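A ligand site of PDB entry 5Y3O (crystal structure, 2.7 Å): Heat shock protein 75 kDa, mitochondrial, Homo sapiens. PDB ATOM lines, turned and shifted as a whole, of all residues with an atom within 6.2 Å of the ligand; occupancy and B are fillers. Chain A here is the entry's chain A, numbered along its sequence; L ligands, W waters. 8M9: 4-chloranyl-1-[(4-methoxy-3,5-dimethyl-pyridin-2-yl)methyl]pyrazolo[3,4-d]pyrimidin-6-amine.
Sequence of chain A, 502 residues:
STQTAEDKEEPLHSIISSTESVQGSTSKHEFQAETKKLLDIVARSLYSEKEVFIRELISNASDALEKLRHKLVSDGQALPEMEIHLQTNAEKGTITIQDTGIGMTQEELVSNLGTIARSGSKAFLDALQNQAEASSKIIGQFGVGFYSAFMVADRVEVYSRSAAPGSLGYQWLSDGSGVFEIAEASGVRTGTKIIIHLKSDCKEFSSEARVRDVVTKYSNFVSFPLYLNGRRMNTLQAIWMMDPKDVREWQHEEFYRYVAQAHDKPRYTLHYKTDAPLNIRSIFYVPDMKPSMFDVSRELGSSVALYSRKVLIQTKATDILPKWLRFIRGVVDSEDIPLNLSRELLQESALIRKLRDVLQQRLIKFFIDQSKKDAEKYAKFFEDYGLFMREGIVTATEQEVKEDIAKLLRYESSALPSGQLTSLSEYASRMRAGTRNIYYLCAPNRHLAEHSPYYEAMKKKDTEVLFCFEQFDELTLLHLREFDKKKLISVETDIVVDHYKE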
ATOM      1  N   PHE A  31       4.805  -0.704 -11.706  1.00  0.00           N
ATOM      2  CA  PHE A  31       4.448  -1.147 -13.045  1.00  0.00           C
ATOM      3  C   PHE A  31       3.142  -0.487 -13.454  1.00  0.00           C
ATOM      4  O   PHE A  31       2.325  -0.117 -12.607  1.00  0.00           O
ATOM      5  CB  PHE A  31       4.312  -2.670 -13.106  1.00  0.00           C
ATOM      6  CG  PHE A  31       5.547  -3.419 -12.667  1.00  0.00           C
ATOM      7  CD1 PHE A  31       5.581  -4.053 -11.435  1.00  0.00           C
ATOM      8  CD2 PHE A  31       6.665  -3.515 -13.486  1.00  0.00           C
ATOM      9  CE1 PHE A  31       6.699  -4.756 -11.020  1.00  0.00           C
ATOM     10  CE2 PHE A  31       7.790  -4.213 -13.077  1.00  0.00           C
ATOM     11  CZ  PHE A  31       7.806  -4.833 -11.835  1.00  0.00           C
ATOM     12  N   LEU A  57      15.681 -16.977 -19.814  1.00  0.00           N
ATOM     13  CA  LEU A  57      16.791 -16.103 -19.482  1.00  0.00           C
ATOM     14  C   LEU A  57      17.997 -16.368 -20.381  1.00  0.00           C
ATOM     15  O   LEU A  57      18.534 -15.446 -20.992  1.00  0.00           O
ATOM     16  CB  LEU A  57      17.162 -16.252 -18.004  1.00  0.00           C
ATOM     17  CG  LEU A  57      16.058 -15.812 -17.047  1.00  0.00           C
ATOM     18  CD1 LEU A  57      16.483 -16.023 -15.603  1.00  0.00           C
ATOM     19  CD2 LEU A  57      15.692 -14.356 -17.299  1.00  0.00           C
ATOM     20  N   ASN A  60      17.391 -14.998 -23.671  1.00  0.00           N
ATOM     21  CA  ASN A  60      17.621 -13.572 -23.610  1.00  0.00           C
ATOM     22  C   ASN A  60      19.115 -13.280 -23.649  1.00  0.00           C
ATOM     23  O   ASN A  60      19.578 -12.445 -24.439  1.00  0.00           O
ATOM     24  CB  ASN A  60      17.005 -12.964 -22.350  1.00  0.00           C
ATOM     25  CG  ASN A  60      15.503 -12.792 -22.458  1.00  0.00           C
ATOM     26  OD1 ASN A  60      14.948 -12.794 -23.560  1.00  0.00           O
ATOM     27  ND2 ASN A  60      14.836 -12.635 -21.318  1.00  0.00           N
ATOM     28  N   ALA A  61      19.871 -14.017 -22.833  1.00  0.00           N
ATOM     29  CA  ALA A  61      21.323 -13.846 -22.763  1.00  0.00           C
ATOM     30  C   ALA A  61      21.948 -14.048 -24.131  1.00  0.00           C
ATOM     31  O   ALA A  61      22.949 -13.403 -24.464  1.00  0.00           O
ATOM     32  CB  ALA A  61      21.930 -14.811 -21.757  1.00  0.00           C
ATOM     33  N   ALA A  64      20.918 -10.674 -26.498  1.00  0.00           N
ATOM     34  CA  ALA A  64      21.810  -9.589 -26.110  1.00  0.00           C
ATOM     35  C   ALA A  64      23.188  -9.784 -26.745  1.00  0.00           C
ATOM     36  O   ALA A  64      23.683  -8.900 -27.446  1.00  0.00           O
ATOM     37  CB  ALA A  64      21.933  -9.510 -24.598  1.00  0.00           C
ATOM     38  N   ASP A  99      25.319 -12.300 -18.499  1.00  0.00           N
ATOM     39  CA  ASP A  99      25.793 -12.208 -19.872  1.00  0.00           C
ATOM     40  C   ASP A  99      26.434 -10.839 -20.055  1.00  0.00           C
ATOM     41  O   ASP A  99      25.938  -9.835 -19.548  1.00  0.00           O
ATOM     42  CB  ASP A  99      24.626 -12.385 -20.855  1.00  0.00           C
ATOM     43  CG  ASP A  99      23.708 -11.191 -20.886  1.00  0.00           C
ATOM     44  OD1 ASP A  99      23.975 -10.255 -21.668  1.00  0.00           O
ATOM     45  OD2 ASP A  99      22.702 -11.182 -20.130  1.00  0.00           O
ATOM     46  N   ILE A 102      25.133  -6.972 -25.048  1.00  0.00           N
ATOM     47  CA  ILE A 102      24.717  -5.575 -25.008  1.00  0.00           C
ATOM     48  C   ILE A 102      23.853  -5.422 -23.760  1.00  0.00           C
ATOM     49  O   ILE A 102      23.230  -6.382 -23.313  1.00  0.00           O
ATOM     50  CB  ILE A 102      23.953  -5.145 -26.276  1.00  0.00           C
ATOM     51  CG1 ILE A 102      24.253  -3.680 -26.615  1.00  0.00           C
ATOM     52  CG2 ILE A 102      22.450  -5.375 -26.129  1.00  0.00           C
ATOM     53  CD1 ILE A 102      23.834  -3.278 -28.012  1.00  0.00           C
ATOM     54  N   GLY A 103      23.847  -4.234 -23.176  1.00  0.00           N
ATOM     55  CA  GLY A 103      23.164  -4.050 -21.918  1.00  0.00           C
ATOM     56  C   GLY A 103      21.836  -3.333 -22.051  1.00  0.00           C
ATOM     57  O   GLY A 103      21.262  -3.254 -23.135  1.00  0.00           O
ATOM     58  N   MET A 104      21.355  -2.819 -20.927  1.00  0.00           N
ATOM     59  CA  MET A 104      20.125  -2.045 -20.919  1.00  0.00           C
ATOM     60  C   MET A 104      20.392  -0.640 -20.420  1.00  0.00           C
ATOM     61  O   MET A 104      20.998  -0.454 -19.369  1.00  0.00           O
ATOM     62  CB  MET A 104      19.074  -2.721 -20.039  1.00  0.00           C
ATOM     63  CG  MET A 104      18.804  -4.170 -20.399  1.00  0.00           C
ATOM     64  SD  MET A 104      17.617  -4.915 -19.286  1.00  0.00           S
ATOM     65  CE  MET A 104      16.172  -3.899 -19.566  1.00  0.00           C
ATOM     66  N   GLU A 108      15.404   1.664 -20.688  1.00  0.00           N
ATOM     67  CA  GLU A 108      14.936   0.300 -20.906  1.00  0.00           C
ATOM     68  C   GLU A 108      14.551  -0.377 -19.597  1.00  0.00           C
ATOM     69  O   GLU A 108      13.549  -1.080 -19.512  1.00  0.00           O
ATOM     70  CB  GLU A 108      16.001  -0.522 -21.636  1.00  0.00           C
ATOM     71  CG  GLU A 108      16.358   0.009 -23.014  1.00  0.00           C
ATOM     72  CD  GLU A 108      17.476  -0.786 -23.670  1.00  0.00           C
ATOM     73  OE1 GLU A 108      17.528  -2.014 -23.465  1.00  0.00           O
ATOM     74  OE2 GLU A 108      18.281  -0.180 -24.398  1.00  0.00           O
ATOM     75  N   LEU A 109      15.363  -0.160 -18.562  1.00  0.00           N
ATOM     76  CA  LEU A 109      15.110  -0.739 -17.254  1.00  0.00           C
ATOM     77  C   LEU A 109      13.839  -0.170 -16.619  1.00  0.00           C
ATOM     78  O   LEU A 109      13.042  -0.911 -16.055  1.00  0.00           O
ATOM     79  CB  LEU A 109      16.298  -0.509 -16.323  1.00  0.00           C
ATOM     80  CG  LEU A 109      17.551  -1.342 -16.606  1.00  0.00           C
ATOM     81  CD1 LEU A 109      18.759  -0.716 -15.967  1.00  0.00           C
ATOM     82  CD2 LEU A 109      17.343  -2.763 -16.107  1.00  0.00           C
ATOM     83  N   SER A 111      11.096   1.433 -18.013  1.00  0.00           N
ATOM     84  CA  SER A 111       9.833   1.137 -18.688  1.00  0.00           C
ATOM     85  C   SER A 111       9.800  -0.299 -19.211  1.00  0.00           C
ATOM     86  O   SER A 111      10.427  -0.629 -20.216  1.00  0.00           O
ATOM     87  CB  SER A 111       9.600   2.116 -19.838  1.00  0.00           C
ATOM     88  OG  SER A 111      10.695   2.124 -20.732  1.00  0.00           O
ATOM     89  N   PHE A 142      12.698  -8.235 -26.927  1.00  0.00           N
ATOM     90  CA  PHE A 142      12.948  -9.464 -26.175  1.00  0.00           C
ATOM     91  C   PHE A 142      11.652 -10.207 -25.874  1.00  0.00           C
ATOM     92  O   PHE A 142      11.466 -11.341 -26.321  1.00  0.00           O
ATOM     93  CB  PHE A 142      13.699  -9.147 -24.870  1.00  0.00           C
ATOM     94  CG  PHE A 142      15.148  -8.847 -25.071  1.00  0.00           C
ATOM     95  CD1 PHE A 142      16.099  -9.852 -24.977  1.00  0.00           C
ATOM     96  CD2 PHE A 142      15.576  -7.557 -25.353  1.00  0.00           C
ATOM     97  CE1 PHE A 142      17.444  -9.578 -25.163  1.00  0.00           C
ATOM     98  CE2 PHE A 142      16.918  -7.275 -25.534  1.00  0.00           C
ATOM     99  CZ  PHE A 142      17.856  -8.283 -25.442  1.00  0.00           C
ATOM    100  N   GLY A 143      10.756  -9.573 -25.123  1.00  0.00           N
ATOM    101  CA  GLY A 143       9.463 -10.161 -24.831  1.00  0.00           C
ATOM    102  C   GLY A 143       9.114 -10.197 -23.360  1.00  0.00           C
ATOM    103  O   GLY A 143       9.294  -9.219 -22.643  1.00  0.00           O
ATOM    104  N   PHE A 146      11.818 -12.899 -19.430  1.00  0.00           N
ATOM    105  CA  PHE A 146      12.426 -12.506 -18.169  1.00  0.00           C
ATOM    106  C   PHE A 146      11.507 -12.714 -16.975  1.00  0.00           C
ATOM    107  O   PHE A 146      11.913 -13.265 -15.953  1.00  0.00           O
ATOM    108  CB  PHE A 146      12.857 -11.033 -18.207  1.00  0.00           C
ATOM    109  CG  PHE A 146      13.277 -10.506 -16.875  1.00  0.00           C
ATOM    110  CD1 PHE A 146      14.507 -10.845 -16.331  1.00  0.00           C
ATOM    111  CD2 PHE A 146      12.430  -9.687 -16.142  1.00  0.00           C
ATOM    112  CE1 PHE A 146      14.894 -10.359 -15.100  1.00  0.00           C
ATOM    113  CE2 PHE A 146      12.810  -9.206 -14.905  1.00  0.00           C
ATOM    114  CZ  PHE A 146      14.042  -9.546 -14.379  1.00  0.00           C
ATOM    115  N   TYR A 147      10.260 -12.267 -17.112  1.00  0.00           N
ATOM    116  CA  TYR A 147       9.322 -12.291 -16.000  1.00  0.00           C
ATOM    117  C   TYR A 147       8.972 -13.711 -15.544  1.00  0.00           C
ATOM    118  O   TYR A 147       8.437 -13.908 -14.447  1.00  0.00           O
ATOM    119  CB  TYR A 147       8.057 -11.525 -16.384  1.00  0.00           C
ATOM    120  CG  TYR A 147       8.327 -10.065 -16.692  1.00  0.00           C
ATOM    121  CD1 TYR A 147       8.479  -9.625 -18.000  1.00  0.00           C
ATOM    122  CD2 TYR A 147       8.453  -9.131 -15.671  1.00  0.00           C
ATOM    123  CE1 TYR A 147       8.738  -8.296 -18.282  1.00  0.00           C
ATOM    124  CE2 TYR A 147       8.711  -7.801 -15.936  1.00  0.00           C
ATOM    125  CZ  TYR A 147       8.855  -7.388 -17.244  1.00  0.00           C
ATOM    126  OH  TYR A 147       9.105  -6.056 -17.516  1.00  0.00           O
ATOM    127  N   VAL A 156      13.853 -10.641  -7.186  1.00  0.00           N
ATOM    128  CA  VAL A 156      14.788 -10.640  -8.303  1.00  0.00           C
ATOM    129  C   VAL A 156      15.642  -9.370  -8.266  1.00  0.00           C
ATOM    130  O   VAL A 156      15.126  -8.246  -8.153  1.00  0.00           O
ATOM    131  CB  VAL A 156      14.042 -10.728  -9.655  1.00  0.00           C
ATOM    132  CG1 VAL A 156      14.992 -10.478 -10.806  1.00  0.00           C
ATOM    133  CG2 VAL A 156      13.363 -12.091  -9.794  1.00  0.00           C
ATOM    134  N   VAL A 158      18.745  -7.402 -10.220  1.00  0.00           N
ATOM    135  CA  VAL A 158      19.354  -7.317 -11.545  1.00  0.00           C
ATOM    136  C   VAL A 158      20.331  -6.153 -11.650  1.00  0.00           C
ATOM    137  O   VAL A 158      20.051  -5.055 -11.195  1.00  0.00           O
ATOM    138  CB  VAL A 158      18.274  -7.180 -12.632  1.00  0.00           C
ATOM    139  CG1 VAL A 158      18.905  -7.168 -14.023  1.00  0.00           C
ATOM    140  CG2 VAL A 158      17.266  -8.304 -12.508  1.00  0.00           C
ATOM    141  N   SER A 160      22.584  -4.137 -14.684  1.00  0.00           N
ATOM    142  CA  SER A 160      22.800  -4.065 -16.133  1.00  0.00           C
ATOM    143  C   SER A 160      23.543  -2.802 -16.541  1.00  0.00           C
ATOM    144  O   SER A 160      23.523  -1.804 -15.827  1.00  0.00           O
ATOM    145  CB  SER A 160      21.465  -4.167 -16.873  1.00  0.00           C
ATOM    146  OG  SER A 160      21.672  -4.487 -18.237  1.00  0.00           O
ATOM    147  N   TRP A 172      18.258  -2.988 -10.381  1.00  0.00           N
ATOM    148  CA  TRP A 172      16.809  -3.123 -10.504  1.00  0.00           C
ATOM    149  C   TRP A 172      16.362  -4.210  -9.532  1.00  0.00           C
ATOM    150  O   TRP A 172      16.851  -5.333  -9.584  1.00  0.00           O
ATOM    151  CB  TRP A 172      16.446  -3.497 -11.950  1.00  0.00           C
ATOM    152  CG  TRP A 172      14.987  -3.680 -12.247  1.00  0.00           C
ATOM    153  CD1 TRP A 172      14.148  -2.783 -12.838  1.00  0.00           C
ATOM    154  CD2 TRP A 172      14.188  -4.851 -12.003  1.00  0.00           C
ATOM    155  NE1 TRP A 172      12.886  -3.305 -12.968  1.00  0.00           N
ATOM    156  CE2 TRP A 172      12.893  -4.580 -12.470  1.00  0.00           C
ATOM    157  CE3 TRP A 172      14.462  -6.107 -11.440  1.00  0.00           C
ATOM    158  CZ2 TRP A 172      11.852  -5.508 -12.377  1.00  0.00           C
ATOM    159  CZ3 TRP A 172      13.434  -7.025 -11.357  1.00  0.00           C
ATOM    160  CH2 TRP A 172      12.147  -6.728 -11.824  1.00  0.00           C
ATOM    161  N   GLY A 191      26.761  -5.648 -20.007  1.00  0.00           N
ATOM    162  CA  GLY A 191      25.889  -6.808 -20.107  1.00  0.00           C
ATOM    163  C   GLY A 191      24.883  -6.824 -18.978  1.00  0.00           C
ATOM    164  O   GLY A 191      24.675  -5.809 -18.311  1.00  0.00           O
ATOM    165  N   THR A 192      24.270  -7.980 -18.734  1.00  0.00           N
ATOM    166  CA  THR A 192      23.220  -8.078 -17.724  1.00  0.00           C
ATOM    167  C   THR A 192      23.489  -9.194 -16.724  1.00  0.00           C
ATOM    168  O   THR A 192      23.811 -10.313 -17.111  1.00  0.00           O
ATOM    169  CB  THR A 192      21.835  -8.290 -18.373  1.00  0.00           C
ATOM    170  OG1 THR A 192      21.504  -7.162 -19.193  1.00  0.00           O
ATOM    171  CG2 THR A 192      20.761  -8.462 -17.316  1.00  0.00           C
ATOM    172  N   LYS A 193      23.335  -8.883 -15.435  1.00  0.00           N
ATOM    173  CA  LYS A 193      23.477  -9.870 -14.387  1.00  0.00           C
ATOM    174  C   LYS A 193      22.173 -10.012 -13.602  1.00  0.00           C
ATOM    175  O   LYS A 193      21.699  -9.045 -13.011  1.00  0.00           O
ATOM    176  CB  LYS A 193      24.619  -9.499 -13.446  1.00  0.00           C
ATOM    177  CG  LYS A 193      24.843 -10.468 -12.297  1.00  0.00           C
ATOM    178  CD  LYS A 193      25.959  -9.963 -11.386  1.00  0.00           C
ATOM    179  CE  LYS A 193      26.199 -10.915 -10.219  1.00  0.00           C
ATOM    180  NZ  LYS A 193      27.348 -10.464  -9.378  1.00  0.00           N
ATOM    181  N   ILE A 194      21.592 -11.206 -13.621  1.00  0.00           N
ATOM    182  CA  ILE A 194      20.328 -11.449 -12.946  1.00  0.00           C
ATOM    183  C   ILE A 194      20.492 -12.391 -11.769  1.00  0.00           C
ATOM    184  O   ILE A 194      20.883 -13.556 -11.928  1.00  0.00           O
ATOM    185  CB  ILE A 194      19.280 -12.043 -13.919  1.00  0.00           C
ATOM    186  CG1 ILE A 194      19.040 -11.091 -15.086  1.00  0.00           C
ATOM    187  CG2 ILE A 194      17.975 -12.325 -13.183  1.00  0.00           C
ATOM    188  CD1 ILE A 194      18.203 -11.693 -16.200  1.00  0.00           C
HETATM  189  C10 8M9 L   1      15.127  -8.917 -19.971  1.00  0.00           C
HETATM  190  C13 8M9 L   1      14.642  -6.383 -17.066  1.00  0.00           C
HETATM  191  C15 8M9 L   1      12.636  -6.593 -18.407  1.00  0.00           C
HETATM  192  C17 8M9 L   1      16.670  -7.790 -17.718  1.00  0.00           C
HETATM  193  C20 8M9 L   1      12.569  -4.984 -16.459  1.00  0.00           C
HETATM  194  N01 8M9 L   1      18.209  -9.423 -20.633  1.00  0.00           N
HETATM  195  C02 8M9 L   1      19.481  -9.458 -21.033  1.00  0.00           C
HETATM  196  N03 8M9 L   1      20.000  -8.537 -21.854  1.00  0.00           N
HETATM  197  C04 8M9 L   1      19.221  -7.534 -22.320  1.00  0.00           C
HETATM  198  C05 8M9 L   1      17.845  -7.450 -21.925  1.00  0.00           C
HETATM  199  C06 8M9 L   1      17.345  -8.452 -21.048  1.00  0.00           C
HETATM  200  C07 8M9 L   1      16.703  -6.568 -22.173  1.00  0.00           C
HETATM  201  N08 8M9 L   1      15.667  -7.070 -21.476  1.00  0.00           N
HETATM  202  N09 8M9 L   1      16.018  -8.152 -20.828  1.00  0.00           N
HETATM  203  C11 8M9 L   1      14.487  -7.876 -19.003  1.00  0.00           C
HETATM  204  C12 8M9 L   1      15.227  -7.340 -17.943  1.00  0.00           C
HETATM  205  C14 8M9 L   1      13.307  -6.012 -17.331  1.00  0.00           C
HETATM  206  N16 8M9 L   1      13.243  -7.490 -19.196  1.00  0.00           N
HETATM  207  O18 8M9 L   1      15.382  -5.817 -15.995  1.00  0.00           O
HETATM  208  C19 8M9 L   1      15.265  -6.461 -14.754  1.00  0.00           C
HETATM  209 CL1  8M9 L   1      19.891  -6.325 -23.401  1.00  0.00          CL
HETATM  210  N22 8M9 L   1      20.311 -10.500 -20.561  1.00  0.00           N
HETATM  211  O   HOH W   1      13.266  -5.256 -21.949  1.00  0.00           O
HETATM  212  O   HOH W   2      21.679 -12.742 -18.313  1.00  0.00           O
HETATM  213  O   HOH W   3      16.919 -11.754 -19.547  1.00  0.00           O
HETATM  214  O   HOH W   4      19.200 -13.196 -19.054  1.00  0.00           O
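The side-chain sulfur (SD) of Met 104 sits close to a nitrogen (N08) of the ligand, 3.6 Å away. Asn 60 touches the ligand. Ala 64 touches the ligand. O of Ile 102 touches CL1 of the ligand, 3.3 Å away. Gly 103 touches the ligand. Leu 109 touches the ligand (CD2 to O18, 3.6 Å). Phe 142 touches the ligand (CE2 to C07, 3.4 Å). CZ of Phe 146 touches C19 of the ligand, 3.3 Å away. Tyr 147 touches the ligand (OH to C15, 3.7 Å). CG2 of Val 158 touches C19 of the ligand, 3.5 Å away. Trp 172 touches the ligand (CD2 to C19, 3.4 Å). 13 residues have an atom within 4 Å of the ligand: Asn 60, Ala 64, Asp 99, Ile 102, Gly 103, Met 104, Leu 109, Phe 142, Phe 146, Tyr 147, Val 158, Trp 172 and Thr 192.
OG of Ser 160 lies within hydrogen-bond range of N of Met 104, at 3.2 Å. The backbone NH (N) of Trp 172 sits at hydrogen-bond distance from the backbone carbonyl oxygen (O) of Val 158 (2.9 Å). The side-chain hydroxyl (OG1) of Thr 192 is in hydrogen-bond range of the side-chain hydroxyl (OG) of Ser 160 (2.8 Å). The backbone NH of Thr 192 sits at hydrogen-bond distance from the backbone carbonyl oxygen of Asp 99 (2.6 Å). The backbone carbonyl oxygen (O) of Ala 64 is in hydrogen-bond range of the backbone NH (N) of Ile 102 (3.4 Å).
A nitrogen (N03) of the ligand lies within hydrogen-bond range of the side-chain hydroxyl (OG1) of Thr 192, at 3.4 Å. OD2 of Asp 99 sits at hydrogen-bond distance from N22 of the ligand (2.5 Å).
Water W3 bridges the side-chain amide nitrogen of Asn 60 (2.9 Å) and a nitrogen (N01) of the ligand (2.9 Å). Water W4 bridges the backbone carbonyl oxygen (O) of Leu 57 (3.0 Å) and a nitrogen (N22) of the ligand (3.3 Å). Water W2 lies within hydrogen-bond range of OD2 of Asp 99 (2.6 Å), O of Thr 192 (3.4 Å) and N22 of the ligand (3.5 Å).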
